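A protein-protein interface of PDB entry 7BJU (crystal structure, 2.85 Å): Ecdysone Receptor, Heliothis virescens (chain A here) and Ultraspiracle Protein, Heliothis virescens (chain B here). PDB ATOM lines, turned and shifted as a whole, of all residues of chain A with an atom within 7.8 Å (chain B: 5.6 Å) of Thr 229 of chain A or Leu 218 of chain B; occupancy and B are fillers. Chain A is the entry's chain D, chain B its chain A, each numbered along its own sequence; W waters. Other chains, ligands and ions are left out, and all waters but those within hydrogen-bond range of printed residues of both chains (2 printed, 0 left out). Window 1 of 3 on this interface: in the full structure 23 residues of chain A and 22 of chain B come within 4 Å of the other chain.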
ATOM      1  N   GLU A 112     -21.423   6.411  -1.980  1.00  0.00           N
ATOM      2  CA  GLU A 112     -20.765   7.016  -0.825  1.00  0.00           C
ATOM      3  C   GLU A 112     -21.501   6.688   0.468  1.00  0.00           C
ATOM      4  O   GLU A 112     -20.872   6.350   1.478  1.00  0.00           O
ATOM      5  CB  GLU A 112     -20.657   8.528  -1.015  1.00  0.00           C
ATOM      6  CG  GLU A 112     -19.759   8.947  -2.167  1.00  0.00           C
ATOM      7  CD  GLU A 112     -19.722  10.451  -2.358  1.00  0.00           C
ATOM      8  OE1 GLU A 112     -20.125  11.181  -1.428  1.00  0.00           O
ATOM      9  OE2 GLU A 112     -19.294  10.905  -3.441  1.00  0.00           O
ATOM     10  N   PHE A 157     -10.949   2.103   5.804  1.00  0.00           N
ATOM     11  CA  PHE A 157     -11.935   3.150   6.042  1.00  0.00           C
ATOM     12  C   PHE A 157     -12.798   2.821   7.253  1.00  0.00           C
ATOM     13  O   PHE A 157     -13.134   3.707   8.048  1.00  0.00           O
ATOM     14  CB  PHE A 157     -12.801   3.344   4.798  1.00  0.00           C
ATOM     15  CG  PHE A 157     -13.871   4.385   4.959  1.00  0.00           C
ATOM     16  CD1 PHE A 157     -13.562   5.733   4.869  1.00  0.00           C
ATOM     17  CD2 PHE A 157     -15.185   4.019   5.197  1.00  0.00           C
ATOM     18  CE1 PHE A 157     -14.543   6.695   5.015  1.00  0.00           C
ATOM     19  CE2 PHE A 157     -16.169   4.977   5.346  1.00  0.00           C
ATOM     20  CZ  PHE A 157     -15.847   6.317   5.256  1.00  0.00           C
ATOM     21  N   LEU A 174     -24.366  13.569   9.020  1.00  0.00           N
ATOM     22  CA  LEU A 174     -23.371  13.380   7.969  1.00  0.00           C
ATOM     23  C   LEU A 174     -23.995  12.769   6.721  1.00  0.00           C
ATOM     24  O   LEU A 174     -23.686  13.185   5.598  1.00  0.00           O
ATOM     25  CB  LEU A 174     -22.231  12.499   8.479  1.00  0.00           C
ATOM     26  CG  LEU A 174     -21.279  11.955   7.411  1.00  0.00           C
ATOM     27  CD1 LEU A 174     -20.447  13.073   6.805  1.00  0.00           C
ATOM     28  CD2 LEU A 174     -20.389  10.859   7.979  1.00  0.00           C
ATOM     29  N   GLY A 222     -14.548  19.338  12.151  1.00  0.00           N
ATOM     30  CA  GLY A 222     -13.679  19.249  10.989  1.00  0.00           C
ATOM     31  C   GLY A 222     -13.396  17.819  10.572  1.00  0.00           C
ATOM     32  O   GLY A 222     -13.340  17.510   9.379  1.00  0.00           O
ATOM     33  N   LYS A 223     -13.214  16.925  11.549  1.00  0.00           N
ATOM     34  CA  LYS A 223     -12.958  15.526  11.226  1.00  0.00           C
ATOM     35  C   LYS A 223     -14.155  14.888  10.532  1.00  0.00           C
ATOM     36  O   LYS A 223     -13.984  14.077   9.612  1.00  0.00           O
ATOM     37  CB  LYS A 223     -12.590  14.749  12.491  1.00  0.00           C
ATOM     38  CG  LYS A 223     -11.238  15.125  13.076  1.00  0.00           C
ATOM     39  CD  LYS A 223     -10.617  13.980  13.862  1.00  0.00           C
ATOM     40  CE  LYS A 223     -11.409  13.646  15.111  1.00  0.00           C
ATOM     41  NZ  LYS A 223     -10.747  12.570  15.905  1.00  0.00           N
ATOM     42  N   ILE A 224     -15.372  15.240  10.952  1.00  0.00           N
ATOM     43  CA  ILE A 224     -16.566  14.694  10.308  1.00  0.00           C
ATOM     44  C   ILE A 224     -16.646  15.165   8.862  1.00  0.00           C
ATOM     45  O   ILE A 224     -16.911  14.378   7.946  1.00  0.00           O
ATOM     46  CB  ILE A 224     -17.828  15.080  11.102  1.00  0.00           C
ATOM     47  CG1 ILE A 224     -17.791  14.443  12.492  1.00  0.00           C
ATOM     48  CG2 ILE A 224     -19.088  14.661  10.353  1.00  0.00           C
ATOM     49  CD1 ILE A 224     -18.937  14.858  13.387  1.00  0.00           C
ATOM     50  N   LEU A 225     -16.410  16.460   8.638  1.00  0.00           N
ATOM     51  CA  LEU A 225     -16.367  16.982   7.277  1.00  0.00           C
ATOM     52  C   LEU A 225     -15.237  16.355   6.473  1.00  0.00           C
ATOM     53  O   LEU A 225     -15.331  16.254   5.244  1.00  0.00           O
ATOM     54  CB  LEU A 225     -16.218  18.503   7.305  1.00  0.00           C
ATOM     55  CG  LEU A 225     -17.363  19.254   7.981  1.00  0.00           C
ATOM     56  CD1 LEU A 225     -17.096  20.749   7.986  1.00  0.00           C
ATOM     57  CD2 LEU A 225     -18.674  18.939   7.286  1.00  0.00           C
ATOM     58  N   GLY A 226     -14.168  15.923   7.145  1.00  0.00           N
ATOM     59  CA  GLY A 226     -13.086  15.248   6.449  1.00  0.00           C
ATOM     60  C   GLY A 226     -13.505  13.931   5.825  1.00  0.00           C
ATOM     61  O   GLY A 226     -12.899  13.487   4.845  1.00  0.00           O
ATOM     62  N   ILE A 227     -14.538  13.289   6.379  1.00  0.00           N
ATOM     63  CA  ILE A 227     -15.040  12.043   5.803  1.00  0.00           C
ATOM     64  C   ILE A 227     -15.590  12.282   4.404  1.00  0.00           C
ATOM     65  O   ILE A 227     -15.476  11.415   3.528  1.00  0.00           O
ATOM     66  CB  ILE A 227     -16.109  11.412   6.720  1.00  0.00           C
ATOM     67  CG1 ILE A 227     -15.565  11.207   8.134  1.00  0.00           C
ATOM     68  CG2 ILE A 227     -16.602  10.087   6.149  1.00  0.00           C
ATOM     69  CD1 ILE A 227     -16.567  10.566   9.074  1.00  0.00           C
ATOM     70  N   LEU A 228     -16.196  13.452   4.173  1.00  0.00           N
ATOM     71  CA  LEU A 228     -16.699  13.783   2.841  1.00  0.00           C
ATOM     72  C   LEU A 228     -15.604  13.648   1.792  1.00  0.00           C
ATOM     73  O   LEU A 228     -15.852  13.168   0.681  1.00  0.00           O
ATOM     74  CB  LEU A 228     -17.267  15.202   2.829  1.00  0.00           C
ATOM     75  CG  LEU A 228     -18.362  15.561   3.833  1.00  0.00           C
ATOM     76  CD1 LEU A 228     -18.724  17.034   3.715  1.00  0.00           C
ATOM     77  CD2 LEU A 228     -19.584  14.699   3.614  1.00  0.00           C
ATOM     78  N   THR A 229     -14.383  14.062   2.133  1.00  0.00           N
ATOM     79  CA  THR A 229     -13.269  13.950   1.200  1.00  0.00           C
ATOM     80  C   THR A 229     -12.917  12.493   0.929  1.00  0.00           C
ATOM     81  O   THR A 229     -12.652  12.115  -0.219  1.00  0.00           O
ATOM     82  CB  THR A 229     -12.052  14.696   1.750  1.00  0.00           C
ATOM     83  OG1 THR A 229     -12.441  16.012   2.160  1.00  0.00           O
ATOM     84  CG2 THR A 229     -10.966  14.805   0.694  1.00  0.00           C
ATOM     85  N   GLU A 230     -12.924  11.655   1.968  1.00  0.00           N
ATOM     86  CA  GLU A 230     -12.428  10.291   1.820  1.00  0.00           C
ATOM     87  C   GLU A 230     -13.413   9.396   1.078  1.00  0.00           C
ATOM     88  O   GLU A 230     -12.996   8.522   0.309  1.00  0.00           O
ATOM     89  CB  GLU A 230     -12.091   9.701   3.190  1.00  0.00           C
ATOM     90  CG  GLU A 230     -10.983  10.446   3.925  1.00  0.00           C
ATOM     91  CD  GLU A 230      -9.711  10.581   3.100  1.00  0.00           C
ATOM     92  OE1 GLU A 230      -9.417   9.678   2.286  1.00  0.00           O
ATOM     93  OE2 GLU A 230      -9.004  11.598   3.267  1.00  0.00           O
ATOM     94  N   ILE A 231     -14.718   9.589   1.286  1.00  0.00           N
ATOM     95  CA  ILE A 231     -15.699   8.778   0.570  1.00  0.00           C
ATOM     96  C   ILE A 231     -15.803   9.158  -0.898  1.00  0.00           C
ATOM     97  O   ILE A 231     -16.398   8.407  -1.679  1.00  0.00           O
ATOM     98  CB  ILE A 231     -17.089   8.858   1.232  1.00  0.00           C
ATOM     99  CG1 ILE A 231     -17.597  10.299   1.261  1.00  0.00           C
ATOM    100  CG2 ILE A 231     -17.044   8.275   2.633  1.00  0.00           C
ATOM    101  CD1 ILE A 231     -18.957  10.438   1.904  1.00  0.00           C
ATOM    102  N   ARG A 232     -15.243  10.305  -1.294  1.00  0.00           N
ATOM    103  CA  ARG A 232     -15.117  10.602  -2.719  1.00  0.00           C
ATOM    104  C   ARG A 232     -14.202   9.594  -3.400  1.00  0.00           C
ATOM    105  O   ARG A 232     -14.463   9.173  -4.533  1.00  0.00           O
ATOM    106  CB  ARG A 232     -14.592  12.023  -2.922  1.00  0.00           C
ATOM    107  CG  ARG A 232     -15.538  13.123  -2.469  1.00  0.00           C
ATOM    108  CD  ARG A 232     -16.831  13.119  -3.271  1.00  0.00           C
ATOM    109  NE  ARG A 232     -17.731  14.190  -2.858  1.00  0.00           N
ATOM    110  CZ  ARG A 232     -17.812  15.372  -3.452  1.00  0.00           C
ATOM    111  NH1 ARG A 232     -17.070  15.669  -4.507  1.00  0.00           N
ATOM    112  NH2 ARG A 232     -18.660  16.280  -2.976  1.00  0.00           N
ATOM    113  N   THR A 233     -13.123   9.193  -2.722  1.00  0.00           N
ATOM    114  CA  THR A 233     -12.222   8.188  -3.276  1.00  0.00           C
ATOM    115  C   THR A 233     -12.910   6.832  -3.374  1.00  0.00           C
ATOM    116  O   THR A 233     -12.804   6.142  -4.394  1.00  0.00           O
ATOM    117  CB  THR A 233     -10.957   8.087  -2.419  1.00  0.00           C
ATOM    118  OG1 THR A 233     -10.330   9.373  -2.336  1.00  0.00           O
ATOM    119  CG2 THR A 233      -9.975   7.089  -3.023  1.00  0.00           C
ATOM    120  N   LEU A 234     -13.627   6.438  -2.317  1.00  0.00           N
ATOM    121  CA  LEU A 234     -14.309   5.147  -2.318  1.00  0.00           C
ATOM    122  C   LEU A 234     -15.380   5.087  -3.399  1.00  0.00           C
ATOM    123  O   LEU A 234     -15.527   4.066  -4.083  1.00  0.00           O
ATOM    124  CB  LEU A 234     -14.917   4.878  -0.940  1.00  0.00           C
ATOM    125  CG  LEU A 234     -13.956   4.956   0.247  1.00  0.00           C
ATOM    126  CD1 LEU A 234     -14.685   4.622   1.538  1.00  0.00           C
ATOM    127  CD2 LEU A 234     -12.764   4.033   0.044  1.00  0.00           C
ATOM    128  N   GLY A 235     -16.138   6.172  -3.571  1.00  0.00           N
ATOM    129  CA  GLY A 235     -17.115   6.212  -4.646  1.00  0.00           C
ATOM    130  C   GLY A 235     -16.474   6.104  -6.015  1.00  0.00           C
ATOM    131  O   GLY A 235     -17.024   5.474  -6.922  1.00  0.00           O
ATOM    132  N   GLU B  85      -3.379  16.984  -5.353  1.00  0.00           N
ATOM    133  CA  GLU B  85      -4.415  17.911  -4.908  1.00  0.00           C
ATOM    134  C   GLU B  85      -3.835  19.290  -4.624  1.00  0.00           C
ATOM    135  O   GLU B  85      -4.480  20.310  -4.887  1.00  0.00           O
ATOM    136  CB  GLU B  85      -5.114  17.361  -3.663  1.00  0.00           C
ATOM    137  CG  GLU B  85      -5.489  15.891  -3.758  1.00  0.00           C
ATOM    138  CD  GLU B  85      -6.197  15.387  -2.517  1.00  0.00           C
ATOM    139  OE1 GLU B  85      -7.250  15.952  -2.159  1.00  0.00           O
ATOM    140  OE2 GLU B  85      -5.697  14.428  -1.894  1.00  0.00           O
ATOM    141  N   PHE B  89      -4.941  22.684  -6.270  1.00  0.00           N
ATOM    142  CA  PHE B  89      -5.383  23.753  -5.378  1.00  0.00           C
ATOM    143  C   PHE B  89      -4.611  25.040  -5.641  1.00  0.00           C
ATOM    144  O   PHE B  89      -5.192  26.132  -5.651  1.00  0.00           O
ATOM    145  CB  PHE B  89      -5.221  23.307  -3.925  1.00  0.00           C
ATOM    146  CG  PHE B  89      -6.015  24.119  -2.943  1.00  0.00           C
ATOM    147  CD1 PHE B  89      -7.361  24.366  -3.156  1.00  0.00           C
ATOM    148  CD2 PHE B  89      -5.421  24.609  -1.791  1.00  0.00           C
ATOM    149  CE1 PHE B  89      -8.097  25.105  -2.248  1.00  0.00           C
ATOM    150  CE2 PHE B  89      -6.151  25.347  -0.876  1.00  0.00           C
ATOM    151  CZ  PHE B  89      -7.491  25.596  -1.105  1.00  0.00           C
ATOM    152  N   LEU B 166      -5.698  25.591   4.556  1.00  0.00           N
ATOM    153  CA  LEU B 166      -6.276  24.455   3.847  1.00  0.00           C
ATOM    154  C   LEU B 166      -5.195  23.578   3.230  1.00  0.00           C
ATOM    155  O   LEU B 166      -5.332  22.350   3.203  1.00  0.00           O
ATOM    156  CB  LEU B 166      -7.258  24.953   2.786  1.00  0.00           C
ATOM    157  CG  LEU B 166      -8.549  25.526   3.374  1.00  0.00           C
ATOM    158  CD1 LEU B 166      -9.364  26.253   2.320  1.00  0.00           C
ATOM    159  CD2 LEU B 166      -9.370  24.419   4.022  1.00  0.00           C
ATOM    160  N   ILE B 169      -4.042  21.392   5.913  1.00  0.00           N
ATOM    161  CA  ILE B 169      -5.067  20.395   6.204  1.00  0.00           C
ATOM    162  C   ILE B 169      -5.081  19.310   5.133  1.00  0.00           C
ATOM    163  O   ILE B 169      -5.296  18.128   5.429  1.00  0.00           O
ATOM    164  CB  ILE B 169      -6.438  21.080   6.352  1.00  0.00           C
ATOM    165  CG1 ILE B 169      -6.462  21.926   7.626  1.00  0.00           C
ATOM    166  CG2 ILE B 169      -7.565  20.059   6.362  1.00  0.00           C
ATOM    167  CD1 ILE B 169      -7.684  22.804   7.757  1.00  0.00           C
ATOM    168  N   ILE B 170      -4.836  19.690   3.876  1.00  0.00           N
ATOM    169  CA  ILE B 170      -4.755  18.704   2.802  1.00  0.00           C
ATOM    170  C   ILE B 170      -3.563  17.780   3.013  1.00  0.00           C
ATOM    171  O   ILE B 170      -3.674  16.556   2.870  1.00  0.00           O
ATOM    172  CB  ILE B 170      -4.684  19.408   1.436  1.00  0.00           C
ATOM    173  CG1 ILE B 170      -5.985  20.154   1.145  1.00  0.00           C
ATOM    174  CG2 ILE B 170      -4.392  18.404   0.334  1.00  0.00           C
ATOM    175  CD1 ILE B 170      -5.835  21.244   0.109  1.00  0.00           C
ATOM    176  N   LEU B 214     -15.366  26.524   3.930  1.00  0.00           N
ATOM    177  CA  LEU B 214     -14.001  26.334   3.451  1.00  0.00           C
ATOM    178  C   LEU B 214     -13.687  24.856   3.257  1.00  0.00           C
ATOM    179  O   LEU B 214     -13.194  24.447   2.198  1.00  0.00           O
ATOM    180  CB  LEU B 214     -13.008  26.967   4.427  1.00  0.00           C
ATOM    181  CG  LEU B 214     -13.086  28.481   4.629  1.00  0.00           C
ATOM    182  CD1 LEU B 214     -12.122  28.931   5.716  1.00  0.00           C
ATOM    183  CD2 LEU B 214     -12.804  29.209   3.324  1.00  0.00           C
ATOM    184  N   LEU B 215     -13.971  24.035   4.272  1.00  0.00           N
ATOM    185  CA  LEU B 215     -13.643  22.616   4.207  1.00  0.00           C
ATOM    186  C   LEU B 215     -14.447  21.877   3.146  1.00  0.00           C
ATOM    187  O   LEU B 215     -14.060  20.771   2.755  1.00  0.00           O
ATOM    188  CB  LEU B 215     -13.866  21.965   5.572  1.00  0.00           C
ATOM    189  CG  LEU B 215     -13.024  22.531   6.718  1.00  0.00           C
ATOM    190  CD1 LEU B 215     -13.400  21.882   8.040  1.00  0.00           C
ATOM    191  CD2 LEU B 215     -11.540  22.352   6.434  1.00  0.00           C
ATOM    192  N   LEU B 216     -15.552  22.456   2.670  1.00  0.00           N
ATOM    193  CA  LEU B 216     -16.332  21.805   1.625  1.00  0.00           C
ATOM    194  C   LEU B 216     -15.618  21.821   0.278  1.00  0.00           C
ATOM    195  O   LEU B 216     -16.013  21.076  -0.627  1.00  0.00           O
ATOM    196  CB  LEU B 216     -17.707  22.461   1.495  1.00  0.00           C
ATOM    197  CG  LEU B 216     -18.714  22.133   2.598  1.00  0.00           C
ATOM    198  CD1 LEU B 216     -19.952  23.006   2.477  1.00  0.00           C
ATOM    199  CD2 LEU B 216     -19.086  20.660   2.557  1.00  0.00           C
ATOM    200  N   ARG B 217     -14.582  22.648   0.122  1.00  0.00           N
ATOM    201  CA  ARG B 217     -13.783  22.608  -1.096  1.00  0.00           C
ATOM    202  C   ARG B 217     -12.905  21.368  -1.156  1.00  0.00           C
ATOM    203  O   ARG B 217     -12.515  20.943  -2.250  1.00  0.00           O
ATOM    204  CB  ARG B 217     -12.909  23.859  -1.210  1.00  0.00           C
ATOM    205  CG  ARG B 217     -13.665  25.181  -1.192  1.00  0.00           C
ATOM    206  CD  ARG B 217     -14.856  25.143  -2.127  1.00  0.00           C
ATOM    207  NE  ARG B 217     -16.108  25.028  -1.391  1.00  0.00           N
ATOM    208  CZ  ARG B 217     -17.223  24.510  -1.887  1.00  0.00           C
ATOM    209  NH1 ARG B 217     -17.268  24.009  -3.112  1.00  0.00           N
ATOM    210  NH2 ARG B 217     -18.319  24.485  -1.133  1.00  0.00           N
ATOM    211  N   LEU B 218     -12.585  20.780   0.001  1.00  0.00           N
ATOM    212  CA  LEU B 218     -11.648  19.658   0.027  1.00  0.00           C
ATOM    213  C   LEU B 218     -12.200  18.414  -0.660  1.00  0.00           C
ATOM    214  O   LEU B 218     -11.462  17.797  -1.448  1.00  0.00           O
ATOM    215  CB  LEU B 218     -11.218  19.378   1.469  1.00  0.00           C
ATOM    216  CG  LEU B 218     -10.585  20.569   2.193  1.00  0.00           C
ATOM    217  CD1 LEU B 218     -10.067  20.158   3.562  1.00  0.00           C
ATOM    218  CD2 LEU B 218      -9.472  21.183   1.356  1.00  0.00           C
ATOM    219  N   PRO B 219     -13.445  17.978  -0.419  1.00  0.00           N
ATOM    220  CA  PRO B 219     -13.963  16.850  -1.214  1.00  0.00           C
ATOM    221  C   PRO B 219     -14.082  17.174  -2.691  1.00  0.00           C
ATOM    222  O   PRO B 219     -13.854  16.298  -3.535  1.00  0.00           O
ATOM    223  CB  PRO B 219     -15.329  16.564  -0.575  1.00  0.00           C
ATOM    224  CG  PRO B 219     -15.696  17.817   0.128  1.00  0.00           C
ATOM    225  CD  PRO B 219     -14.406  18.386   0.621  1.00  0.00           C
ATOM    226  N   ALA B 220     -14.436  18.416  -3.029  1.00  0.00           N
ATOM    227  CA  ALA B 220     -14.430  18.826  -4.428  1.00  0.00           C
ATOM    228  C   ALA B 220     -13.026  18.743  -5.014  1.00  0.00           C
ATOM    229  O   ALA B 220     -12.845  18.301  -6.154  1.00  0.00           O
ATOM    230  CB  ALA B 220     -14.987  20.243  -4.563  1.00  0.00           C
ATOM    231  N   LEU B 221     -12.018  19.156  -4.242  1.00  0.00           N
ATOM    232  CA  LEU B 221     -10.638  19.034  -4.698  1.00  0.00           C
ATOM    233  C   LEU B 221     -10.232  17.576  -4.866  1.00  0.00           C
ATOM    234  O   LEU B 221      -9.452  17.249  -5.768  1.00  0.00           O
ATOM    235  CB  LEU B 221      -9.701  19.742  -3.719  1.00  0.00           C
ATOM    236  CG  LEU B 221      -8.207  19.695  -4.038  1.00  0.00           C
ATOM    237  CD1 LEU B 221      -7.939  20.225  -5.437  1.00  0.00           C
ATOM    238  CD2 LEU B 221      -7.420  20.485  -3.012  1.00  0.00           C
ATOM    239  N   ARG B 222     -10.753  16.688  -4.017  1.00  0.00           N
ATOM    240  CA  ARG B 222     -10.395  15.275  -4.106  1.00  0.00           C
ATOM    241  C   ARG B 222     -10.924  14.651  -5.392  1.00  0.00           C
ATOM    242  O   ARG B 222     -10.185  13.971  -6.112  1.00  0.00           O
ATOM    243  CB  ARG B 222     -10.922  14.526  -2.882  1.00  0.00           C
ATOM    244  CG  ARG B 222     -10.734  13.019  -2.932  1.00  0.00           C
ATOM    245  CD  ARG B 222      -9.273  12.626  -2.784  1.00  0.00           C
ATOM    246  NE  ARG B 222      -8.727  13.006  -1.486  1.00  0.00           N
ATOM    247  CZ  ARG B 222      -8.739  12.229  -0.413  1.00  0.00           C
ATOM    248  NH1 ARG B 222      -9.271  11.017  -0.441  1.00  0.00           N
ATOM    249  NH2 ARG B 222      -8.201  12.676   0.719  1.00  0.00           N
ATOM    250  N   SER B 223     -12.206  14.875  -5.700  1.00  0.00           N
ATOM    251  CA  SER B 223     -12.789  14.305  -6.912  1.00  0.00           C
ATOM    252  C   SER B 223     -12.063  14.789  -8.161  1.00  0.00           C
ATOM    253  O   SER B 223     -11.770  13.996  -9.064  1.00  0.00           O
ATOM    254  CB  SER B 223     -14.276  14.647  -6.996  1.00  0.00           C
ATOM    255  OG  SER B 223     -14.999  14.075  -5.921  1.00  0.00           O
HETATM  256  O   HOH W   1     -18.396  19.631  -2.113  1.00  0.00           O
HETATM  257  O   HOH W   2     -13.558  18.437   4.420  1.00  0.00           O
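Of the 15 printed residues of chain B, 6 touch a printed residue of chain A. Hydrophobic or aromatic side chains of chain B within 4 Å of the printed part of chain A: Leu 215, Leu 216, Leu 218 and Pro 219. Hydrophobic or aromatic side chains of chain A within 4 Å of the printed part of chain B: Leu 225 and Leu 228. Among the printed residues, 12 pairs touch across the chains. Among the printed residues, Asp or Glu carboxylates within 4 Å of a Lys or Arg side-chain nitrogen of the other chain: Glu 230 of chain A with Arg 222 of chain B (2.9 Å).
Gly 222 of chain A touches Leu 215 of chain B (CA to CD1, 3.96 Å). Leu 225 of chain A touches Leu 215 of chain B (CD1 to CD1, 3.9 Å). Leu 228 of chain A touches Leu 216 of chain B. Leu 228 of chain A touches Pro 219 of chain B (O to CB, 3.7 Å). OG1 of Thr 229 of chain A touches CB of Leu 218 of chain B (3.6 Å). Arg 222 of chain B touches Thr 229 of chain A. CB of Arg 232 of chain A touches CG of Arg 222 of chain B (3.98 Å).
Printed residues of chain B within 4 Å of Leu 225 of chain A: Leu 215. Of the printed residues of chain B, Leu 228 of chain A touches Leu 216 (3.8 Å) and Pro 219 (3.7 Å). Leu 218 of chain B touches just one residue of chain A: Thr 229 (3.6 Å). Pro 219 of chain B touches just these residues of chain A: Leu 228 (3.7 Å), Thr 229 (3.4 Å) and Arg 232 (3.4 Å). The nearest residue of chain A that does not touch Leu 218 of chain B is Arg 232 of chain A (6.3 Å).
OE1 of Glu 85 of chain B is in salt-bridge range of NE of Arg 222 of chain B, at 3.4 Å. The backbone carbonyl oxygen (O) of Pro 219 of chain B is in hydrogen-bond range of the side-chain hydroxyl (OG) of Ser 223 of chain B (3.5 Å). NE of Arg 232 of chain A lies within salt-bridge range of OE2 of Glu 112 of chain A, at 3.7 Å.
NH1 of Arg 232 of chain A sits at hydrogen-bond distance from O of Pro 219 of chain B (3.4 Å). NH2 of Arg 222 of chain B lies within salt-bridge range of OE2 of Glu 230 of chain A (2.9 Å). NH1 of Arg 222 of chain B sits at hydrogen-bond distance from OG1 of Thr 233 of chain A (2.7 Å). The side-chain hydroxyl of Ser 223 of chain B is in hydrogen-bond range of the guanidinium group of Arg 232 of chain A. The backbone nitrogen (N) of Pro 219 of chain B sits close to the side-chain hydroxyl (OG1) of Thr 229 of chain A.
Water W2 lies within hydrogen-bond range of O of Leu 215 of chain B, O of Leu 225 of chain A and OG1 of Thr 229 of chain A. Water W1 bridges the backbone carbonyl oxygen (O) of Leu 216 of chain B and the guanidinium group (NH2) of Arg 232 of chain A.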
